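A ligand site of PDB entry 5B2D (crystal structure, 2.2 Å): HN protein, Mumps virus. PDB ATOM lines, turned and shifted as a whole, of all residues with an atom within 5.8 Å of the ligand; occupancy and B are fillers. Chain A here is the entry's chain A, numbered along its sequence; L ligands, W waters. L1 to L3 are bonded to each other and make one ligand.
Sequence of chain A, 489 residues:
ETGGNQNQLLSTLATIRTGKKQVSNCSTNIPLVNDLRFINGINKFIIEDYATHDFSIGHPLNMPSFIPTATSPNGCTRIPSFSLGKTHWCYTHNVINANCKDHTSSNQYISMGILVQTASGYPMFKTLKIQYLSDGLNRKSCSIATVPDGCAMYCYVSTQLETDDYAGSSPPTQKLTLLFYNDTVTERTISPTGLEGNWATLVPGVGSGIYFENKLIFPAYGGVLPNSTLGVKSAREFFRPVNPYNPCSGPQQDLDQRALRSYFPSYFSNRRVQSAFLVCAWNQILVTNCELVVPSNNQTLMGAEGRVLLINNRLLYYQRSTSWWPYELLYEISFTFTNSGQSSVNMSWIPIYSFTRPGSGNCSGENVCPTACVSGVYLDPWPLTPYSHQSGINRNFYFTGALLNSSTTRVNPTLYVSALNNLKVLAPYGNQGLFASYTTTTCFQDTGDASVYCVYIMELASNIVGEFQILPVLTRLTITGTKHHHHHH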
ATOM      1  N   ARG A  78      16.264 -19.801  15.565  1.00  0.00           N
ATOM      2  CA  ARG A  78      14.875 -19.979  15.977  1.00  0.00           C
ATOM      3  C   ARG A  78      14.420 -21.441  15.966  1.00  0.00           C
ATOM      4  O   ARG A  78      15.142 -22.318  15.527  1.00  0.00           O
ATOM      5  CB  ARG A  78      13.953 -19.161  15.065  1.00  0.00           C
ATOM      6  CG  ARG A  78      13.858 -17.672  15.371  1.00  0.00           C
ATOM      7  CD  ARG A  78      12.509 -17.151  14.961  1.00  0.00           C
ATOM      8  NE  ARG A  78      11.457 -17.681  15.826  1.00  0.00           N
ATOM      9  CZ  ARG A  78      10.175 -17.733  15.498  1.00  0.00           C
ATOM     10  NH1 ARG A  78       9.765 -17.288  14.319  1.00  0.00           N
ATOM     11  NH2 ARG A  78       9.302 -18.231  16.364  1.00  0.00           N
ATOM     12  N   ILE A  79      13.189 -21.668  16.443  1.00  0.00           N
ATOM     13  CA  ILE A  79      12.474 -22.944  16.334  1.00  0.00           C
ATOM     14  C   ILE A  79      13.146 -24.109  17.083  1.00  0.00           C
ATOM     15  O   ILE A  79      13.592 -25.093  16.464  1.00  0.00           O
ATOM     16  CB  ILE A  79      12.283 -23.345  14.838  1.00  0.00           C
ATOM     17  CG1 ILE A  79      11.889 -22.133  13.987  1.00  0.00           C
ATOM     18  CG2 ILE A  79      11.235 -24.447  14.702  1.00  0.00           C
ATOM     19  CD1 ILE A  79      10.644 -21.433  14.441  1.00  0.00           C
ATOM     20  N   LYS A 140      13.424 -26.994   7.406  1.00  0.00           N
ATOM     21  CA  LYS A 140      12.799 -26.175   8.435  1.00  0.00           C
ATOM     22  C   LYS A 140      11.576 -26.855   9.073  1.00  0.00           C
ATOM     23  O   LYS A 140      11.106 -27.895   8.608  1.00  0.00           O
ATOM     24  CB  LYS A 140      12.422 -24.792   7.900  1.00  0.00           C
ATOM     25  CG  LYS A 140      11.376 -24.746   6.827  1.00  0.00           C
ATOM     26  CD  LYS A 140      11.143 -23.311   6.365  1.00  0.00           C
ATOM     27  CE  LYS A 140      10.226 -22.518   7.289  1.00  0.00           C
ATOM     28  NZ  LYS A 140       9.819 -21.184   6.707  1.00  0.00           N
ATOM     29  N   SER A 141      11.146 -26.277  10.191  1.00  0.00           N
ATOM     30  CA  SER A 141      10.046 -26.776  11.013  1.00  0.00           C
ATOM     31  C   SER A 141      10.369 -28.144  11.624  1.00  0.00           C
ATOM     32  O   SER A 141       9.473 -28.930  11.882  1.00  0.00           O
ATOM     33  CB  SER A 141       8.753 -26.847  10.193  1.00  0.00           C
ATOM     34  OG  SER A 141       7.609 -26.840  11.024  1.00  0.00           O
ATOM     35  N   TYR A 156      11.013 -30.774   6.695  1.00  0.00           N
ATOM     36  CA  TYR A 156      10.645 -30.694   5.298  1.00  0.00           C
ATOM     37  C   TYR A 156      11.621 -29.726   4.652  1.00  0.00           C
ATOM     38  O   TYR A 156      12.225 -28.890   5.336  1.00  0.00           O
ATOM     39  CB  TYR A 156       9.186 -30.260   5.108  1.00  0.00           C
ATOM     40  CG  TYR A 156       8.916 -28.773   5.181  1.00  0.00           C
ATOM     41  CD1 TYR A 156       8.917 -28.106   6.392  1.00  0.00           C
ATOM     42  CD2 TYR A 156       8.611 -28.050   4.034  1.00  0.00           C
ATOM     43  CE1 TYR A 156       8.662 -26.753   6.461  1.00  0.00           C
ATOM     44  CE2 TYR A 156       8.357 -26.694   4.089  1.00  0.00           C
ATOM     45  CZ  TYR A 156       8.388 -26.050   5.306  1.00  0.00           C
ATOM     46  OH  TYR A 156       8.120 -24.701   5.373  1.00  0.00           O
ATOM     47  N   GLU A 162       5.380 -20.378   2.984  1.00  0.00           N
ATOM     48  CA  GLU A 162       4.436 -21.335   3.541  1.00  0.00           C
ATOM     49  C   GLU A 162       3.068 -21.206   2.874  1.00  0.00           C
ATOM     50  O   GLU A 162       2.378 -22.199   2.618  1.00  0.00           O
ATOM     51  CB  GLU A 162       4.288 -21.120   5.055  1.00  0.00           C
ATOM     52  CG  GLU A 162       3.333 -22.092   5.711  1.00  0.00           C
ATOM     53  CD  GLU A 162       3.052 -21.747   7.167  1.00  0.00           C
ATOM     54  OE1 GLU A 162       3.125 -20.558   7.530  1.00  0.00           O
ATOM     55  OE2 GLU A 162       2.750 -22.673   7.943  1.00  0.00           O
ATOM     56  N   TYR A 166       0.784 -23.941   0.770  1.00  0.00           N
ATOM     57  CA  TYR A 166      -0.641 -24.320   0.874  1.00  0.00           C
ATOM     58  C   TYR A 166      -1.441 -24.046  -0.391  1.00  0.00           C
ATOM     59  O   TYR A 166      -2.447 -24.703  -0.649  1.00  0.00           O
ATOM     60  CB  TYR A 166      -1.309 -23.619   2.052  1.00  0.00           C
ATOM     61  CG  TYR A 166      -0.991 -24.223   3.399  1.00  0.00           C
ATOM     62  CD1 TYR A 166       0.194 -23.933   4.041  1.00  0.00           C
ATOM     63  CD2 TYR A 166      -1.878 -25.093   4.026  1.00  0.00           C
ATOM     64  CE1 TYR A 166       0.500 -24.474   5.274  1.00  0.00           C
ATOM     65  CE2 TYR A 166      -1.592 -25.642   5.263  1.00  0.00           C
ATOM     66  CZ  TYR A 166      -0.394 -25.334   5.881  1.00  0.00           C
ATOM     67  OH  TYR A 166      -0.074 -25.870   7.116  1.00  0.00           O
ATOM     68  N   VAL A 203       4.199 -30.503   7.005  1.00  0.00           N
ATOM     69  CA  VAL A 203       5.440 -30.143   7.671  1.00  0.00           C
ATOM     70  C   VAL A 203       5.439 -30.758   9.057  1.00  0.00           C
ATOM     71  O   VAL A 203       4.399 -31.104   9.584  1.00  0.00           O
ATOM     72  CB  VAL A 203       5.632 -28.615   7.782  1.00  0.00           C
ATOM     73  CG1 VAL A 203       5.413 -27.923   6.437  1.00  0.00           C
ATOM     74  CG2 VAL A 203       4.691 -28.048   8.820  1.00  0.00           C
ATOM     75  N   TYR A 221       1.653 -31.311  10.679  1.00  0.00           N
ATOM     76  CA  TYR A 221       0.417 -30.652  10.250  1.00  0.00           C
ATOM     77  C   TYR A 221       0.544 -30.148   8.823  1.00  0.00           C
ATOM     78  O   TYR A 221       1.648 -30.035   8.295  1.00  0.00           O
ATOM     79  CB  TYR A 221       0.045 -29.499  11.204  1.00  0.00           C
ATOM     80  CG  TYR A 221       0.973 -28.309  11.140  1.00  0.00           C
ATOM     81  CD1 TYR A 221       2.221 -28.345  11.746  1.00  0.00           C
ATOM     82  CD2 TYR A 221       0.598 -27.144  10.471  1.00  0.00           C
ATOM     83  CE1 TYR A 221       3.065 -27.249  11.695  1.00  0.00           C
ATOM     84  CE2 TYR A 221       1.433 -26.062  10.418  1.00  0.00           C
ATOM     85  CZ  TYR A 221       2.665 -26.113  11.012  1.00  0.00           C
ATOM     86  OH  TYR A 221       3.507 -25.029  10.953  1.00  0.00           O
ATOM     87  N   TYR A 267      -6.029 -17.611   4.424  1.00  0.00           N
ATOM     88  CA  TYR A 267      -4.584 -17.403   4.468  1.00  0.00           C
ATOM     89  C   TYR A 267      -3.848 -18.623   3.905  1.00  0.00           C
ATOM     90  O   TYR A 267      -2.817 -18.491   3.265  1.00  0.00           O
ATOM     91  CB  TYR A 267      -4.137 -17.107   5.901  1.00  0.00           C
ATOM     92  CG  TYR A 267      -2.664 -16.827   6.052  1.00  0.00           C
ATOM     93  CD1 TYR A 267      -2.101 -15.661   5.561  1.00  0.00           C
ATOM     94  CD2 TYR A 267      -1.826 -17.730   6.714  1.00  0.00           C
ATOM     95  CE1 TYR A 267      -0.757 -15.394   5.698  1.00  0.00           C
ATOM     96  CE2 TYR A 267      -0.473 -17.471   6.857  1.00  0.00           C
ATOM     97  CZ  TYR A 267       0.062 -16.303   6.349  1.00  0.00           C
ATOM     98  OH  TYR A 267       1.400 -16.036   6.478  1.00  0.00           O
ATOM     99  N   PHE A 268      -4.392 -19.807   4.158  1.00  0.00           N
ATOM    100  CA  PHE A 268      -3.817 -21.051   3.670  1.00  0.00           C
ATOM    101  C   PHE A 268      -4.599 -21.623   2.478  1.00  0.00           C
ATOM    102  O   PHE A 268      -4.589 -22.831   2.256  1.00  0.00           O
ATOM    103  CB  PHE A 268      -3.727 -22.073   4.808  1.00  0.00           C
ATOM    104  CG  PHE A 268      -2.598 -21.777   5.769  1.00  0.00           C
ATOM    105  CD1 PHE A 268      -1.488 -21.068   5.362  1.00  0.00           C
ATOM    106  CD2 PHE A 268      -2.653 -22.221   7.082  1.00  0.00           C
ATOM    107  CE1 PHE A 268      -0.441 -20.800   6.224  1.00  0.00           C
ATOM    108  CE2 PHE A 268      -1.611 -21.946   7.960  1.00  0.00           C
ATOM    109  CZ  PHE A 268      -0.505 -21.236   7.531  1.00  0.00           C
ATOM    110  N   GLY A 303      -5.325 -27.834  12.431  1.00  0.00           N
ATOM    111  CA  GLY A 303      -3.958 -28.322  12.446  1.00  0.00           C
ATOM    112  C   GLY A 303      -2.927 -27.268  12.753  1.00  0.00           C
ATOM    113  O   GLY A 303      -3.016 -26.123  12.288  1.00  0.00           O
ATOM    114  N   ALA A 304      -1.940 -27.644  13.553  1.00  0.00           N
ATOM    115  CA  ALA A 304      -0.924 -26.717  13.990  1.00  0.00           C
ATOM    116  C   ALA A 304       0.316 -27.449  14.501  1.00  0.00           C
ATOM    117  O   ALA A 304       0.334 -28.680  14.579  1.00  0.00           O
ATOM    118  CB  ALA A 304      -1.476 -25.804  15.076  1.00  0.00           C
ATOM    119  N   GLU A 305       1.340 -26.679  14.842  1.00  0.00           N
ATOM    120  CA  GLU A 305       2.514 -27.219  15.513  1.00  0.00           C
ATOM    121  C   GLU A 305       2.083 -27.948  16.760  1.00  0.00           C
ATOM    122  O   GLU A 305       1.019 -27.696  17.306  1.00  0.00           O
ATOM    123  CB  GLU A 305       3.478 -26.096  15.860  1.00  0.00           C
ATOM    124  CG  GLU A 305       4.164 -25.475  14.664  1.00  0.00           C
ATOM    125  CD  GLU A 305       4.903 -24.219  15.009  1.00  0.00           C
ATOM    126  OE1 GLU A 305       4.659 -23.668  16.106  1.00  0.00           O
ATOM    127  OE2 GLU A 305       5.730 -23.786  14.201  1.00  0.00           O
ATOM    128  N   ARG A 320      -0.470 -26.481  19.339  1.00  0.00           N
ATOM    129  CA  ARG A 320      -0.361 -25.027  19.373  1.00  0.00           C
ATOM    130  C   ARG A 320      -1.714 -24.400  19.050  1.00  0.00           C
ATOM    131  O   ARG A 320      -2.443 -24.896  18.184  1.00  0.00           O
ATOM    132  CB  ARG A 320       0.709 -24.532  18.411  1.00  0.00           C
ATOM    133  CG  ARG A 320       0.636 -23.058  18.100  1.00  0.00           C
ATOM    134  CD  ARG A 320       1.713 -22.666  17.123  1.00  0.00           C
ATOM    135  NE  ARG A 320       1.431 -21.387  16.480  1.00  0.00           N
ATOM    136  CZ  ARG A 320       2.345 -20.647  15.864  1.00  0.00           C
ATOM    137  NH1 ARG A 320       3.609 -21.048  15.818  1.00  0.00           N
ATOM    138  NH2 ARG A 320       1.988 -19.509  15.286  1.00  0.00           N
ATOM    139  N   THR A 322      -3.197 -22.145  17.140  1.00  0.00           N
ATOM    140  CA  THR A 322      -3.081 -21.330  15.940  1.00  0.00           C
ATOM    141  C   THR A 322      -4.461 -20.831  15.530  1.00  0.00           C
ATOM    142  O   THR A 322      -4.599 -19.771  14.926  1.00  0.00           O
ATOM    143  CB  THR A 322      -2.438 -22.131  14.809  1.00  0.00           C
ATOM    144  OG1 THR A 322      -1.166 -22.620  15.260  1.00  0.00           O
ATOM    145  CG2 THR A 322      -2.240 -21.291  13.556  1.00  0.00           C
ATOM    146  N   VAL A 374      -5.168 -17.885  11.668  1.00  0.00           N
ATOM    147  CA  VAL A 374      -3.818 -18.435  11.693  1.00  0.00           C
ATOM    148  C   VAL A 374      -2.988 -17.474  12.541  1.00  0.00           C
ATOM    149  O   VAL A 374      -2.566 -16.413  12.070  1.00  0.00           O
ATOM    150  CB  VAL A 374      -3.215 -18.599  10.297  1.00  0.00           C
ATOM    151  CG1 VAL A 374      -1.809 -19.147  10.392  1.00  0.00           C
ATOM    152  CG2 VAL A 374      -4.078 -19.542   9.470  1.00  0.00           C
ATOM    153  N   SER A 375      -2.754 -17.850  13.792  1.00  0.00           N
ATOM    154  CA  SER A 375      -2.210 -16.933  14.785  1.00  0.00           C
ATOM    155  C   SER A 375      -1.513 -17.705  15.898  1.00  0.00           C
ATOM    156  O   SER A 375      -1.069 -18.827  15.704  1.00  0.00           O
ATOM    157  CB  SER A 375      -3.316 -16.048  15.360  1.00  0.00           C
ATOM    158  OG  SER A 375      -2.774 -14.932  16.024  1.00  0.00           O
ATOM    159  N   GLY A 376      -1.411 -17.072  17.063  1.00  0.00           N
ATOM    160  CA  GLY A 376      -0.921 -17.755  18.242  1.00  0.00           C
ATOM    161  C   GLY A 376       0.575 -17.939  18.230  1.00  0.00           C
ATOM    162  O   GLY A 376       1.277 -17.268  17.468  1.00  0.00           O
ATOM    163  N   VAL A 377       1.064 -18.827  19.075  1.00  0.00           N
ATOM    164  CA  VAL A 377       2.488 -19.037  19.247  1.00  0.00           C
ATOM    165  C   VAL A 377       2.682 -20.405  19.917  1.00  0.00           C
ATOM    166  O   VAL A 377       1.765 -20.897  20.600  1.00  0.00           O
ATOM    167  CB  VAL A 377       3.124 -17.898  20.088  1.00  0.00           C
ATOM    168  CG1 VAL A 377       2.437 -17.781  21.441  1.00  0.00           C
ATOM    169  CG2 VAL A 377       4.640 -18.063  20.247  1.00  0.00           C
ATOM    170  N   ARG A 410       4.094 -10.858  21.493  1.00  0.00           N
ATOM    171  CA  ARG A 410       4.978 -11.897  22.001  1.00  0.00           C
ATOM    172  C   ARG A 410       6.021 -11.249  22.886  1.00  0.00           C
ATOM    173  O   ARG A 410       7.098 -10.846  22.435  1.00  0.00           O
ATOM    174  CB  ARG A 410       5.635 -12.669  20.854  1.00  0.00           C
ATOM    175  CG  ARG A 410       4.664 -13.477  20.001  1.00  0.00           C
ATOM    176  CD  ARG A 410       5.368 -14.100  18.810  1.00  0.00           C
ATOM    177  NE  ARG A 410       4.488 -15.019  18.093  1.00  0.00           N
ATOM    178  CZ  ARG A 410       4.873 -15.811  17.103  1.00  0.00           C
ATOM    179  NH1 ARG A 410       6.153 -15.812  16.710  1.00  0.00           N
ATOM    180  NH2 ARG A 410       4.003 -16.614  16.513  1.00  0.00           N
ATOM    181  N   TYR A 438       8.646 -18.643  21.067  1.00  0.00           N
ATOM    182  CA  TYR A 438       8.439 -20.065  21.366  1.00  0.00           C
ATOM    183  C   TYR A 438       9.004 -20.485  22.715  1.00  0.00           C
ATOM    184  O   TYR A 438      10.074 -20.037  23.119  1.00  0.00           O
ATOM    185  CB  TYR A 438       9.069 -20.939  20.279  1.00  0.00           C
ATOM    186  CG  TYR A 438       8.304 -21.044  18.980  1.00  0.00           C
ATOM    187  CD1 TYR A 438       7.393 -20.073  18.603  1.00  0.00           C
ATOM    188  CD2 TYR A 438       8.481 -22.142  18.152  1.00  0.00           C
ATOM    189  CE1 TYR A 438       6.694 -20.178  17.418  1.00  0.00           C
ATOM    190  CE2 TYR A 438       7.785 -22.257  16.967  1.00  0.00           C
ATOM    191  CZ  TYR A 438       6.892 -21.282  16.613  1.00  0.00           C
ATOM    192  OH  TYR A 438       6.189 -21.401  15.434  1.00  0.00           O
HETATM  193  C1  LIG L   1      -0.089 -12.356   9.057  1.00  0.00           C
HETATM  194  C2  LIG L   1       1.276 -11.855   9.534  1.00  0.00           C
HETATM  195  C3  LIG L   1       2.324 -12.865   9.387  1.00  0.00           C
HETATM  196  C4  LIG L   1       1.947 -14.137   9.980  1.00  0.00           C
HETATM  197  C5  LIG L   1       0.632 -14.630   9.402  1.00  0.00           C
HETATM  198  C6  LIG L   1       0.251 -15.966  10.071  1.00  0.00           C
HETATM  199  O1  LIG L   1      -0.087 -12.434   7.658  1.00  0.00           O
HETATM  200  O2  LIG L   1       1.635 -10.675   8.766  1.00  0.00           O
HETATM  201  O3  LIG L   1       3.576 -12.363  10.061  1.00  0.00           O
HETATM  202  O4  LIG L   1       3.011 -15.150   9.734  1.00  0.00           O
HETATM  203  O5  LIG L   1      -0.428 -13.674   9.604  1.00  0.00           O
HETATM  204  O6  LIG L   1       0.014 -15.747  11.462  1.00  0.00           O
HETATM  205  C1  LG2 L   2       3.717 -15.384  10.924  1.00  0.00           C
HETATM  206  C2  LG2 L   2       4.479 -16.724  10.813  1.00  0.00           C
HETATM  207  C3  LG2 L   2       5.392 -16.936  11.984  1.00  0.00           C
HETATM  208  C4  LG2 L   2       6.282 -15.760  12.202  1.00  0.00           C
HETATM  209  C5  LG2 L   2       5.490 -14.478  12.344  1.00  0.00           C
HETATM  210  C6  LG2 L   2       6.456 -13.329  12.472  1.00  0.00           C
HETATM  211  O1  LG2 L   2       3.537 -17.798  10.757  1.00  0.00           O
HETATM  212  O2  LG2 L   2       6.244 -18.132  11.746  1.00  0.00           O
HETATM  213  O3  LG2 L   2       7.161 -15.635  11.085  1.00  0.00           O
HETATM  214  O4  LG2 L   2       4.609 -14.236  11.196  1.00  0.00           O
HETATM  215  O5  LG2 L   2       5.909 -12.348  13.368  1.00  0.00           O
HETATM  216  C1  LG3 L   3       5.954 -18.341  14.057  1.00  0.00           C
HETATM  217  C2  LG3 L   3       6.046 -19.200  12.855  1.00  0.00           C
HETATM  218  C3  LG3 L   3       7.259 -20.066  12.891  1.00  0.00           C
HETATM  219  C4  LG3 L   3       7.429 -20.978  11.739  1.00  0.00           C
HETATM  220  C5  LG3 L   3       6.196 -21.150  10.952  1.00  0.00           C
HETATM  221  C6  LG3 L   3       4.984 -21.161  11.824  1.00  0.00           C
HETATM  222  C7  LG3 L   3       3.765 -21.375  10.981  1.00  0.00           C
HETATM  223  C8  LG3 L   3       2.548 -21.498  11.886  1.00  0.00           C
HETATM  224  C9  LG3 L   3       1.292 -21.427  11.055  1.00  0.00           C
HETATM  225  C10 LG3 L   3       6.398 -22.518   8.798  1.00  0.00           C
HETATM  226  C11 LG3 L   3       6.458 -23.866   8.107  1.00  0.00           C
HETATM  227  N1  LG3 L   3       6.273 -22.459  10.254  1.00  0.00           N
HETATM  228  O1  LG3 L   3       6.973 -17.824  14.539  1.00  0.00           O
HETATM  229  O2  LG3 L   3       4.838 -18.234  14.676  1.00  0.00           O
HETATM  230  O3  LG3 L   3       8.487 -20.467  10.871  1.00  0.00           O
HETATM  231  O4  LG3 L   3       4.823 -19.899  12.578  1.00  0.00           O
HETATM  232  O5  LG3 L   3       3.585 -20.279  10.127  1.00  0.00           O
HETATM  233  O6  LG3 L   3       2.600 -22.714  12.566  1.00  0.00           O
HETATM  234  O7  LG3 L   3       1.124 -22.658  10.317  1.00  0.00           O
HETATM  235  O8  LG3 L   3       6.445 -21.495   8.148  1.00  0.00           O
HETATM  236  O   HOH W   1       6.037 -24.809  11.881  1.00  0.00           O
HETATM  237  O   HOH W   2       0.757 -23.788  13.851  1.00  0.00           O
HETATM  238  O   HOH W   3       6.060 -18.875   7.602  1.00  0.00           O
HETATM  239  O   HOH W   4      -1.080 -24.032  11.614  1.00  0.00           O
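Water W2 lies within hydrogen-bond range of O6 of LG3 L3, OG1 of Thr 322 and N of Glu 305.
Water W3 bridges an oxygen (O8) of LG3 L3 (2.7 Å) and the side-chain carboxylate (OE1) of Glu 162 (3.4 Å).
Water W1 lies within hydrogen-bond range of the side-chain carboxylate of Glu 305, the side-chain hydroxyl of Tyr 221, the side-chain hydroxyl of Ser 141 and a nitrogen (N1) of LG3 L3.
Water W4 lies within hydrogen-bond range of an oxygen (O7) of LG3 L3 (2.9 Å) and the backbone carbonyl oxygen (O) of Gly 303 (2.9 Å).
NH1 of Arg 320 lies within salt-bridge range of OE1 of Glu 305 (2.8 Å).
O of Gly 376 lies within hydrogen-bond range of NH2 of Arg 410, 3.0 Å away.
The backbone NH of Lys 140 lies within hydrogen-bond range of the backbone carbonyl oxygen of Tyr 156, 3.1 Å away.
The guanidinium group (NE) of Arg 320 is in hydrogen-bond range of the side-chain hydroxyl (OG1) of Thr 322 (3.1 Å).
The backbone carbonyl oxygen (O) of Tyr 221 is in hydrogen-bond range of the backbone NH (N) of Val 203.
The guanidinium group (NH1) of Arg 320 sits at hydrogen-bond distance from the side-chain hydroxyl (OH) of Tyr 438 (2.6 Å).
The guanidinium group (NH2) of Arg 320 lies within hydrogen-bond range of the backbone carbonyl oxygen (O) of Ser 375 (3.2 Å).
The side-chain hydroxyl of Tyr 438 lies within hydrogen-bond range of the side-chain carboxylate of Glu 305, 2.7 Å away.
NH1 of Arg 78 is in salt-bridge range of O1 of LG3 L3.
An oxygen (O2) of LG3 L3 lies within salt-bridge range of the guanidinium group (NH2) of Arg 320 (3.2 Å).
The backbone carbonyl oxygen (O) of Val 374 lies within hydrogen-bond range of an oxygen (O6) of LIG L1 (2.7 Å).
OH of Tyr 221 sits at hydrogen-bond distance from O6 of LG3 L3 (3.0 Å).
The side-chain carboxylate (OE1) of Glu 162 is in hydrogen-bond range of an oxygen (O5) of LG3 L3.
The guanidinium group of Arg 410 lies within salt-bridge range of an oxygen (O2) of LG3 L3 (2.6 Å).
CD1 of Ile 79 touches C3 of LG3 L3, 3.97 Å away.
NZ of Lys 140 touches O8 of LG3 L3, at 3.7 Å.
OH of Tyr 156 touches C11 of LG3 L3, 3.3 Å away.
OH of Tyr 267 touches C5 of LIG L1, at 3.3 Å.
CZ of Phe 268 touches O7 of LG3 L3, at 3.5 Å.
OE2 of Glu 305 touches C6 of LG3 L3 (3.6 Å).
OH of Tyr 438 touches C3 of LG3 L3 (3.1 Å).
Hydrophobic or aromatic side chains that line the ligand: Ile 79, Tyr 156, Tyr 221, Tyr 267, Phe 268, Val 374 and Tyr 438.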
